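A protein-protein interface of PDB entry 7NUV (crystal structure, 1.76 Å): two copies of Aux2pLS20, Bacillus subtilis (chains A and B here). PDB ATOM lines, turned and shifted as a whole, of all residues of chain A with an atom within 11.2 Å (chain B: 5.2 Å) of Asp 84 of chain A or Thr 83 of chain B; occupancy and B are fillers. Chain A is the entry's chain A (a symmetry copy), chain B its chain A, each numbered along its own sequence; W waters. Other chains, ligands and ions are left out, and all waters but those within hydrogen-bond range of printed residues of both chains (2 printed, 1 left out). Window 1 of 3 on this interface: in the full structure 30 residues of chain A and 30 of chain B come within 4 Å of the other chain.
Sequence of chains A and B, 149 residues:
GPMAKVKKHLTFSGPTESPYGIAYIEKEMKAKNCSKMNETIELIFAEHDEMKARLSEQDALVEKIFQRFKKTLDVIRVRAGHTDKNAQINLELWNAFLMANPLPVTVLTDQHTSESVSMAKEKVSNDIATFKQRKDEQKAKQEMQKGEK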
ATOM      1  N   VAL A  75      20.887 -19.333  40.541  1.00  0.00           N
ATOM      2  CA  VAL A  75      21.974 -18.911  39.658  1.00  0.00           C
ATOM      3  C   VAL A  75      21.462 -18.621  38.255  1.00  0.00           C
ATOM      4  O   VAL A  75      21.858 -17.630  37.632  1.00  0.00           O
ATOM      5  CB  VAL A  75      23.074 -19.984  39.641  1.00  0.00           C
ATOM      6  CG1 VAL A  75      24.011 -19.780  38.475  1.00  0.00           C
ATOM      7  CG2 VAL A  75      23.845 -19.910  40.939  1.00  0.00           C
ATOM      8  N   ILE A  76      20.633 -19.514  37.705  1.00  0.00           N
ATOM      9  CA  ILE A  76      20.111 -19.281  36.360  1.00  0.00           C
ATOM     10  C   ILE A  76      19.279 -18.007  36.323  1.00  0.00           C
ATOM     11  O   ILE A  76      19.450 -17.161  35.439  1.00  0.00           O
ATOM     12  CB  ILE A  76      19.312 -20.501  35.865  1.00  0.00           C
ATOM     13  CG1 ILE A  76      20.228 -21.717  35.659  1.00  0.00           C
ATOM     14  CG2 ILE A  76      18.512 -20.171  34.596  1.00  0.00           C
ATOM     15  CD1 ILE A  76      19.457 -23.022  35.645  1.00  0.00           C
ATOM     16  N   ARG A  77      18.349 -17.858  37.272  1.00  0.00           N
ATOM     17  CA  ARG A  77      17.572 -16.627  37.350  1.00  0.00           C
ATOM     18  C   ARG A  77      18.447 -15.384  37.401  1.00  0.00           C
ATOM     19  O   ARG A  77      18.166 -14.400  36.706  1.00  0.00           O
ATOM     20  CB  ARG A  77      16.630 -16.659  38.549  1.00  0.00           C
ATOM     21  CG  ARG A  77      15.618 -15.522  38.522  1.00  0.00           C
ATOM     22  CD  ARG A  77      14.755 -15.474  39.767  1.00  0.00           C
ATOM     23  NE  ARG A  77      15.498 -15.506  41.018  1.00  0.00           N
ATOM     24  CZ  ARG A  77      15.107 -16.203  42.076  1.00  0.00           C
ATOM     25  NH1 ARG A  77      13.993 -16.919  42.054  1.00  0.00           N
ATOM     26  NH2 ARG A  77      15.855 -16.194  43.176  1.00  0.00           N
ATOM     27  N   VAL A  78      19.498 -15.399  38.223  1.00  0.00           N
ATOM     28  CA  VAL A  78      20.335 -14.207  38.364  1.00  0.00           C
ATOM     29  C   VAL A  78      21.100 -13.936  37.075  1.00  0.00           C
ATOM     30  O   VAL A  78      21.205 -12.786  36.617  1.00  0.00           O
ATOM     31  CB  VAL A  78      21.282 -14.373  39.562  1.00  0.00           C
ATOM     32  CG1 VAL A  78      22.476 -13.419  39.444  1.00  0.00           C
ATOM     33  CG2 VAL A  78      20.521 -14.180  40.848  1.00  0.00           C
ATOM     34  N   ARG A  79      21.652 -14.985  36.468  1.00  0.00           N
ATOM     35  CA  ARG A  79      22.344 -14.808  35.195  1.00  0.00           C
ATOM     36  C   ARG A  79      21.409 -14.261  34.114  1.00  0.00           C
ATOM     37  O   ARG A  79      21.763 -13.323  33.379  1.00  0.00           O
ATOM     38  CB  ARG A  79      22.973 -16.131  34.764  1.00  0.00           C
ATOM     39  CG  ARG A  79      24.242 -16.483  35.536  1.00  0.00           C
ATOM     40  CD  ARG A  79      25.030 -17.547  34.779  1.00  0.00           C
ATOM     41  NE  ARG A  79      26.370 -17.723  35.325  1.00  0.00           N
ATOM     42  CZ  ARG A  79      26.998 -18.880  35.433  1.00  0.00           C
ATOM     43  NH1 ARG A  79      26.463 -20.003  34.977  1.00  0.00           N
ATOM     44  NH2 ARG A  79      28.224 -18.902  35.947  1.00  0.00           N
ATOM     45  N   ALA A  80      20.204 -14.825  34.005  1.00  0.00           N
ATOM     46  CA  ALA A  80      19.258 -14.343  33.002  1.00  0.00           C
ATOM     47  C   ALA A  80      18.915 -12.879  33.218  1.00  0.00           C
ATOM     48  O   ALA A  80      18.707 -12.144  32.247  1.00  0.00           O
ATOM     49  CB  ALA A  80      17.982 -15.182  33.011  1.00  0.00           C
ATOM     50  N   GLY A  81      18.852 -12.434  34.475  1.00  0.00           N
ATOM     51  CA  GLY A  81      18.643 -11.018  34.734  1.00  0.00           C
ATOM     52  C   GLY A  81      19.810 -10.167  34.261  1.00  0.00           C
ATOM     53  O   GLY A  81      19.610  -9.067  33.735  1.00  0.00           O
ATOM     54  N   HIS A  82      21.042 -10.639  34.477  1.00  0.00           N
ATOM     55  CA  HIS A  82      22.211  -9.912  33.978  1.00  0.00           C
ATOM     56  C   HIS A  82      22.202  -9.784  32.462  1.00  0.00           C
ATOM     57  O   HIS A  82      22.495  -8.711  31.919  1.00  0.00           O
ATOM     58  CB  HIS A  82      23.530 -10.585  34.384  1.00  0.00           C
ATOM     59  CG  HIS A  82      23.782 -10.645  35.853  1.00  0.00           C
ATOM     60  ND1 HIS A  82      23.236  -9.744  36.743  1.00  0.00           N
ATOM     61  CD2 HIS A  82      24.601 -11.443  36.576  1.00  0.00           C
ATOM     62  CE1 HIS A  82      23.668 -10.019  37.961  1.00  0.00           C
ATOM     63  NE2 HIS A  82      24.505 -11.039  37.886  1.00  0.00           N
ATOM     64  N   THR A  83      21.925 -10.876  31.752  1.00  0.00           N
ATOM     65  CA  THR A  83      22.004 -10.762  30.308  1.00  0.00           C
ATOM     66  C   THR A  83      20.789 -10.035  29.761  1.00  0.00           C
ATOM     67  O   THR A  83      20.909  -9.318  28.768  1.00  0.00           O
ATOM     68  CB  THR A  83      22.185 -12.130  29.650  1.00  0.00           C
ATOM     69  OG1 THR A  83      20.965 -12.871  29.713  1.00  0.00           O
ATOM     70  CG2 THR A  83      23.248 -12.887  30.369  1.00  0.00           C
ATOM     71  N   ASP A  84      19.629 -10.158  30.419  1.00  0.00           N
ATOM     72  CA  ASP A  84      18.508  -9.289  30.069  1.00  0.00           C
ATOM     73  C   ASP A  84      18.916  -7.822  30.166  1.00  0.00           C
ATOM     74  O   ASP A  84      18.695  -7.041  29.233  1.00  0.00           O
ATOM     75  CB  ASP A  84      17.307  -9.602  30.975  1.00  0.00           C
ATOM     76  CG  ASP A  84      16.008  -8.888  30.547  1.00  0.00           C
ATOM     77  OD1 ASP A  84      15.919  -8.352  29.422  1.00  0.00           O
ATOM     78  OD2 ASP A  84      15.049  -8.881  31.354  1.00  0.00           O
ATOM     79  N   LYS A  85      19.556  -7.440  31.278  1.00  0.00           N
ATOM     80  CA  LYS A  85      20.004  -6.057  31.447  1.00  0.00           C
ATOM     81  C   LYS A  85      21.004  -5.660  30.361  1.00  0.00           C
ATOM     82  O   LYS A  85      20.876  -4.596  29.743  1.00  0.00           O
ATOM     83  CB  LYS A  85      20.618  -5.874  32.837  1.00  0.00           C
ATOM     84  CG  LYS A  85      21.219  -4.492  33.033  1.00  0.00           C
ATOM     85  CD  LYS A  85      21.526  -4.190  34.501  1.00  0.00           C
ATOM     86  CE  LYS A  85      22.177  -2.825  34.610  1.00  0.00           C
ATOM     87  NZ  LYS A  85      22.356  -2.370  36.041  1.00  0.00           N
ATOM     88  N   ASN A  86      22.010  -6.508  30.114  1.00  0.00           N
ATOM     89  CA  ASN A  86      22.997  -6.203  29.079  1.00  0.00           C
ATOM     90  C   ASN A  86      22.364  -6.094  27.697  1.00  0.00           C
ATOM     91  O   ASN A  86      22.760  -5.239  26.890  1.00  0.00           O
ATOM     92  CB  ASN A  86      24.099  -7.257  29.093  1.00  0.00           C
ATOM     93  CG  ASN A  86      25.132  -6.965  30.153  1.00  0.00           C
ATOM     94  OD1 ASN A  86      25.182  -5.843  30.663  1.00  0.00           O
ATOM     95  ND2 ASN A  86      25.939  -7.960  30.512  1.00  0.00           N
ATOM     96  N   ALA A  87      21.398  -6.955  27.394  1.00  0.00           N
ATOM     97  CA  ALA A  87      20.743  -6.871  26.086  1.00  0.00           C
ATOM     98  C   ALA A  87      19.968  -5.564  25.921  1.00  0.00           C
ATOM     99  O   ALA A  87      19.914  -5.014  24.813  1.00  0.00           O
ATOM    100  CB  ALA A  87      19.836  -8.083  25.885  1.00  0.00           C
ATOM    101  N   GLN A  88      19.387  -5.039  27.009  1.00  0.00           N
ATOM    102  CA  GLN A  88      18.739  -3.728  26.984  1.00  0.00           C
ATOM    103  C   GLN A  88      19.739  -2.598  26.752  1.00  0.00           C
ATOM    104  O   GLN A  88      19.482  -1.692  25.951  1.00  0.00           O
ATOM    105  CB  GLN A  88      17.977  -3.504  28.296  1.00  0.00           C
ATOM    106  CG  GLN A  88      16.792  -4.451  28.477  1.00  0.00           C
ATOM    107  CD  GLN A  88      16.090  -4.284  29.833  1.00  0.00           C
ATOM    108  OE1 GLN A  88      15.681  -3.186  30.231  1.00  0.00           O
ATOM    109  NE2 GLN A  88      15.922  -5.402  30.535  1.00  0.00           N
ATOM    110  N   ILE A  89      20.881  -2.643  27.443  1.00  0.00           N
ATOM    111  CA  ILE A  89      21.948  -1.668  27.230  1.00  0.00           C
ATOM    112  C   ILE A  89      22.440  -1.717  25.807  1.00  0.00           C
ATOM    113  O   ILE A  89      22.681  -0.676  25.181  1.00  0.00           O
ATOM    114  CB  ILE A  89      23.098  -1.914  28.223  1.00  0.00           C
ATOM    115  CG1 ILE A  89      22.596  -1.696  29.664  1.00  0.00           C
ATOM    116  CG2 ILE A  89      24.330  -1.086  27.853  1.00  0.00           C
ATOM    117  CD1 ILE A  89      23.582  -2.160  30.752  1.00  0.00           C
ATOM    118  N   ASN A  90      22.601  -2.925  25.268  1.00  0.00           N
ATOM    119  CA  ASN A  90      23.049  -3.063  23.890  1.00  0.00           C
ATOM    120  C   ASN A  90      22.105  -2.354  22.920  1.00  0.00           C
ATOM    121  O   ASN A  90      22.552  -1.677  21.984  1.00  0.00           O
ATOM    122  CB  ASN A  90      23.188  -4.550  23.546  1.00  0.00           C
ATOM    123  CG  ASN A  90      23.468  -4.767  22.085  1.00  0.00           C
ATOM    124  OD1 ASN A  90      24.609  -4.595  21.676  1.00  0.00           O
ATOM    125  ND2 ASN A  90      22.457  -5.179  21.291  1.00  0.00           N
ATOM    126  N   LEU A  91      20.794  -2.476  23.138  1.00  0.00           N
ATOM    127  CA  LEU A  91      19.842  -1.830  22.241  1.00  0.00           C
ATOM    128  C   LEU A  91      19.890  -0.306  22.366  1.00  0.00           C
ATOM    129  O   LEU A  91      19.713   0.408  21.369  1.00  0.00           O
ATOM    130  CB  LEU A  91      18.435  -2.362  22.520  1.00  0.00           C
ATOM    131  CG  LEU A  91      17.790  -3.177  21.401  1.00  0.00           C
ATOM    132  CD1 LEU A  91      17.207  -2.264  20.329  1.00  0.00           C
ATOM    133  CD2 LEU A  91      18.796  -4.120  20.775  1.00  0.00           C
ATOM    134  N   GLU A  92      20.131   0.213  23.578  1.00  0.00           N
ATOM    135  CA  GLU A  92      20.259   1.662  23.761  1.00  0.00           C
ATOM    136  C   GLU A  92      21.462   2.209  23.002  1.00  0.00           C
ATOM    137  O   GLU A  92      21.399   3.306  22.424  1.00  0.00           O
ATOM    138  CB  GLU A  92      20.393   2.003  25.251  1.00  0.00           C
ATOM    139  CG  GLU A  92      19.150   1.700  26.070  1.00  0.00           C
ATOM    140  CD  GLU A  92      17.985   2.540  25.655  1.00  0.00           C
ATOM    141  OE1 GLU A  92      16.843   2.066  25.756  1.00  0.00           O
ATOM    142  OE2 GLU A  92      18.216   3.690  25.226  1.00  0.00           O
ATOM    143  N   ARG B  79      12.184 -14.234  30.978  1.00  0.00           N
ATOM    144  CA  ARG B  79      13.431 -13.524  30.707  1.00  0.00           C
ATOM    145  C   ARG B  79      14.122 -14.055  29.449  1.00  0.00           C
ATOM    146  O   ARG B  79      14.572 -13.276  28.591  1.00  0.00           O
ATOM    147  CB  ARG B  79      14.349 -13.616  31.923  1.00  0.00           C
ATOM    148  CG  ARG B  79      13.939 -12.693  33.068  1.00  0.00           C
ATOM    149  CD  ARG B  79      15.106 -12.515  34.033  1.00  0.00           C
ATOM    150  NE  ARG B  79      14.864 -11.441  34.989  1.00  0.00           N
ATOM    151  CZ  ARG B  79      15.226 -11.462  36.259  1.00  0.00           C
ATOM    152  NH1 ARG B  79      15.920 -12.470  36.764  1.00  0.00           N
ATOM    153  NH2 ARG B  79      14.947 -10.411  37.025  1.00  0.00           N
ATOM    154  N   ALA B  80      14.209 -15.380  29.312  1.00  0.00           N
ATOM    155  CA  ALA B  80      14.846 -15.953  28.129  1.00  0.00           C
ATOM    156  C   ALA B  80      14.130 -15.540  26.855  1.00  0.00           C
ATOM    157  O   ALA B  80      14.775 -15.346  25.819  1.00  0.00           O
ATOM    158  CB  ALA B  80      14.897 -17.476  28.225  1.00  0.00           C
ATOM    159  N   GLY B  81      12.803 -15.396  26.905  1.00  0.00           N
ATOM    160  CA  GLY B  81      12.085 -14.889  25.747  1.00  0.00           C
ATOM    161  C   GLY B  81      12.446 -13.448  25.429  1.00  0.00           C
ATOM    162  O   GLY B  81      12.562 -13.076  24.256  1.00  0.00           O
ATOM    163  N   HIS B  82      12.588 -12.608  26.459  1.00  0.00           N
ATOM    164  CA  HIS B  82      13.014 -11.225  26.233  1.00  0.00           C
ATOM    165  C   HIS B  82      14.392 -11.147  25.593  1.00  0.00           C
ATOM    166  O   HIS B  82      14.610 -10.358  24.664  1.00  0.00           O
ATOM    167  CB  HIS B  82      13.055 -10.411  27.534  1.00  0.00           C
ATOM    168  CG  HIS B  82      11.739 -10.243  28.215  1.00  0.00           C
ATOM    169  ND1 HIS B  82      10.537 -10.292  27.542  1.00  0.00           N
ATOM    170  CD2 HIS B  82      11.443  -9.931  29.498  1.00  0.00           C
ATOM    171  CE1 HIS B  82       9.551 -10.069  28.394  1.00  0.00           C
ATOM    172  NE2 HIS B  82      10.075  -9.837  29.585  1.00  0.00           N
ATOM    173  N   THR B  83      15.354 -11.912  26.103  1.00  0.00           N
ATOM    174  CA  THR B  83      16.683 -11.766  25.539  1.00  0.00           C
ATOM    175  C   THR B  83      16.774 -12.461  24.194  1.00  0.00           C
ATOM    176  O   THR B  83      17.498 -11.989  23.317  1.00  0.00           O
ATOM    177  CB  THR B  83      17.757 -12.267  26.506  1.00  0.00           C
ATOM    178  OG1 THR B  83      17.736 -13.694  26.566  1.00  0.00           O
ATOM    179  CG2 THR B  83      17.490 -11.721  27.866  1.00  0.00           C
ATOM    180  N   ASP B  84      16.011 -13.542  23.988  1.00  0.00           N
ATOM    181  CA  ASP B  84      15.888 -14.090  22.639  1.00  0.00           C
ATOM    182  C   ASP B  84      15.402 -13.017  21.668  1.00  0.00           C
ATOM    183  O   ASP B  84      15.996 -12.813  20.602  1.00  0.00           O
ATOM    184  CB  ASP B  84      14.946 -15.303  22.656  1.00  0.00           C
ATOM    185  CG  ASP B  84      14.916 -16.080  21.324  1.00  0.00           C
ATOM    186  OD1 ASP B  84      15.787 -15.879  20.451  1.00  0.00           O
ATOM    187  OD2 ASP B  84      14.005 -16.925  21.157  1.00  0.00           O
ATOM    188  N   LYS B  85      14.344 -12.289  22.044  1.00  0.00           N
ATOM    189  CA  LYS B  85      13.823 -11.225  21.185  1.00  0.00           C
ATOM    190  C   LYS B  85      14.875 -10.142  20.943  1.00  0.00           C
ATOM    191  O   LYS B  85      15.100  -9.723  19.801  1.00  0.00           O
ATOM    192  CB  LYS B  85      12.563 -10.621  21.809  1.00  0.00           C
ATOM    193  CG  LYS B  85      12.041  -9.424  21.031  1.00  0.00           C
ATOM    194  CD  LYS B  85      10.622  -9.031  21.443  1.00  0.00           C
ATOM    195  CE  LYS B  85      10.196  -7.797  20.672  1.00  0.00           C
ATOM    196  NZ  LYS B  85       8.742  -7.440  20.887  1.00  0.00           N
ATOM    197  N   ASN B  86      15.532  -9.676  22.012  1.00  0.00           N
ATOM    198  CA  ASN B  86      16.562  -8.649  21.857  1.00  0.00           C
ATOM    199  C   ASN B  86      17.722  -9.126  20.990  1.00  0.00           C
ATOM    200  O   ASN B  86      18.272  -8.351  20.194  1.00  0.00           O
ATOM    201  CB  ASN B  86      17.056  -8.205  23.230  1.00  0.00           C
ATOM    202  CG  ASN B  86      16.136  -7.178  23.843  1.00  0.00           C
ATOM    203  OD1 ASN B  86      15.315  -6.592  23.133  1.00  0.00           O
ATOM    204  ND2 ASN B  86      16.242  -6.966  25.153  1.00  0.00           N
ATOM    205  N   ALA B  87      18.121 -10.386  21.137  1.00  0.00           N
ATOM    206  CA  ALA B  87      19.215 -10.896  20.306  1.00  0.00           C
ATOM    207  C   ALA B  87      18.836 -10.930  18.826  1.00  0.00           C
ATOM    208  O   ALA B  87      19.692 -10.691  17.965  1.00  0.00           O
ATOM    209  CB  ALA B  87      19.639 -12.277  20.802  1.00  0.00           C
ATOM    210  N   GLN B  88      17.561 -11.196  18.512  1.00  0.00           N
ATOM    211  CA  GLN B  88      17.069 -11.119  17.136  1.00  0.00           C
ATOM    212  C   GLN B  88      17.092  -9.691  16.598  1.00  0.00           C
ATOM    213  O   GLN B  88      17.517  -9.459  15.460  1.00  0.00           O
ATOM    214  CB  GLN B  88      15.649 -11.694  17.062  1.00  0.00           C
ATOM    215  CG  GLN B  88      15.588 -13.193  17.348  1.00  0.00           C
ATOM    216  CD  GLN B  88      14.155 -13.745  17.364  1.00  0.00           C
ATOM    217  OE1 GLN B  88      13.373 -13.570  16.420  1.00  0.00           O
ATOM    218  NE2 GLN B  88      13.821 -14.449  18.442  1.00  0.00           N
HETATM  219  O   HOH W   1      20.283  -6.509  22.306  1.00  0.00           O
HETATM  220  O   HOH W   2      20.645 -14.955  27.248  1.00  0.00           O
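Water W1 lies within hydrogen-bond range of ND2 of Asn 90 of chain A (2.7 Å), O of Ala 87 of chain A (2.9 Å) and O of Asn 86 of chain B (3.4 Å).
Water W2 bridges the side-chain hydroxyl (OG1) of Thr 83 of chain B (3.2 Å) and the side-chain hydroxyl (OG1) of Thr 83 of chain A (3.2 Å).
Ala 80 of chain A touches Arg 79 of chain B, but with the chains exchanged Arg 79 of chain A does not touch Ala 80 of chain B (8.7 Å).
Gly 81 of chain A touches Arg 79 of chain B, but with the chains exchanged Arg 79 of chain A does not touch Gly 81 of chain B (11.2 Å).
Asp 84 of chain A touches Thr 83 of chain B, but with the chains exchanged Thr 83 of chain A does not touch Asp 84 of chain B (7.6 Å).
Ala 87 of chain A touches Asn 86 of chain B, but with the chains exchanged Asn 86 of chain A does not touch Ala 87 of chain B (8.9 Å).
Positions printed for both chains: 79, 80, 81, 82, 83, 84, 85, 86, 87 and 88.
Of the 5 pairs that touch across the chains among the printed residues, none has its exchanged pair printed and touching as well.
Of the 10 printed residues of chain B, 3 touch a printed residue of chain A.
Printed residues of chain B that touch a printed residue of chain A: Arg 79, Thr 83 and Asn 86.
Along chain B the printed residues that touch a printed residue of chain A span positions 79 to 86.
Of the 18 printed residues of chain A, 5 touch a printed residue of chain B.
Among the printed residues, 5 pairs touch across the chains.
Among the printed residues, no Asp or Glu carboxylate lies within 4 Å of a Lys or Arg side-chain nitrogen of the other chain.
OD1 of Asp 84 of chain A is in hydrogen-bond range of NE2 of Gln 88 of chain A.
O of Ala 80 of chain A is in hydrogen-bond range of OG1 of Thr 83 of chain A, at 3.5 Å.
The backbone carbonyl oxygen of Ala 80 of chain B is in hydrogen-bond range of the side-chain hydroxyl of Thr 83 of chain B, 3.5 Å away.
Printed residues of chain B within 4 Å of Arg 77 of chain A: Arg 79 (3.0 Å).
Of the printed residues of chain B, Ala 80 of chain A touches Arg 79.
Printed residues of chain B within 4 Å of Gly 81 of chain A: Arg 79 (3.7 Å).
Printed residues of chain B within 4 Å of Asp 84 of chain A: Thr 83 (3.4 Å).
Printed residues of chain B within 4 Å of Ala 87 of chain A: Asn 86.
No residue of chain A comes within 4 Å of Gly 81 of chain B.
Of the printed residues of chain A, Thr 83 of chain B touches Asp 84.
No residue of chain A comes within 4 Å of Asp 84 of chain B.
Asn 86 of chain B touches just one residue of chain A: Ala 87 (3.8 Å).
No residue of chain A comes within 4 Å of Ala 87 of chain B.
The nearest printed residue of chain A that does not touch Thr 83 of chain B is Thr 83 of chain A (4.1 Å).
Arg 79 of chain B touches Ala 80 of chain A (CD to C, 3.9 Å).
Arg 79 of chain B touches Gly 81 of chain A (NH1 to CA, 3.7 Å).
CA of Asp 84 of chain A touches CG2 of Thr 83 of chain B, 3.4 Å away.
Ala 87 of chain A touches Asn 86 of chain B (CB to ND2, 3.8 Å).
O of Arg 77 of chain A lies within hydrogen-bond range of NH1 of Arg 79 of chain B, 3.0 Å away.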
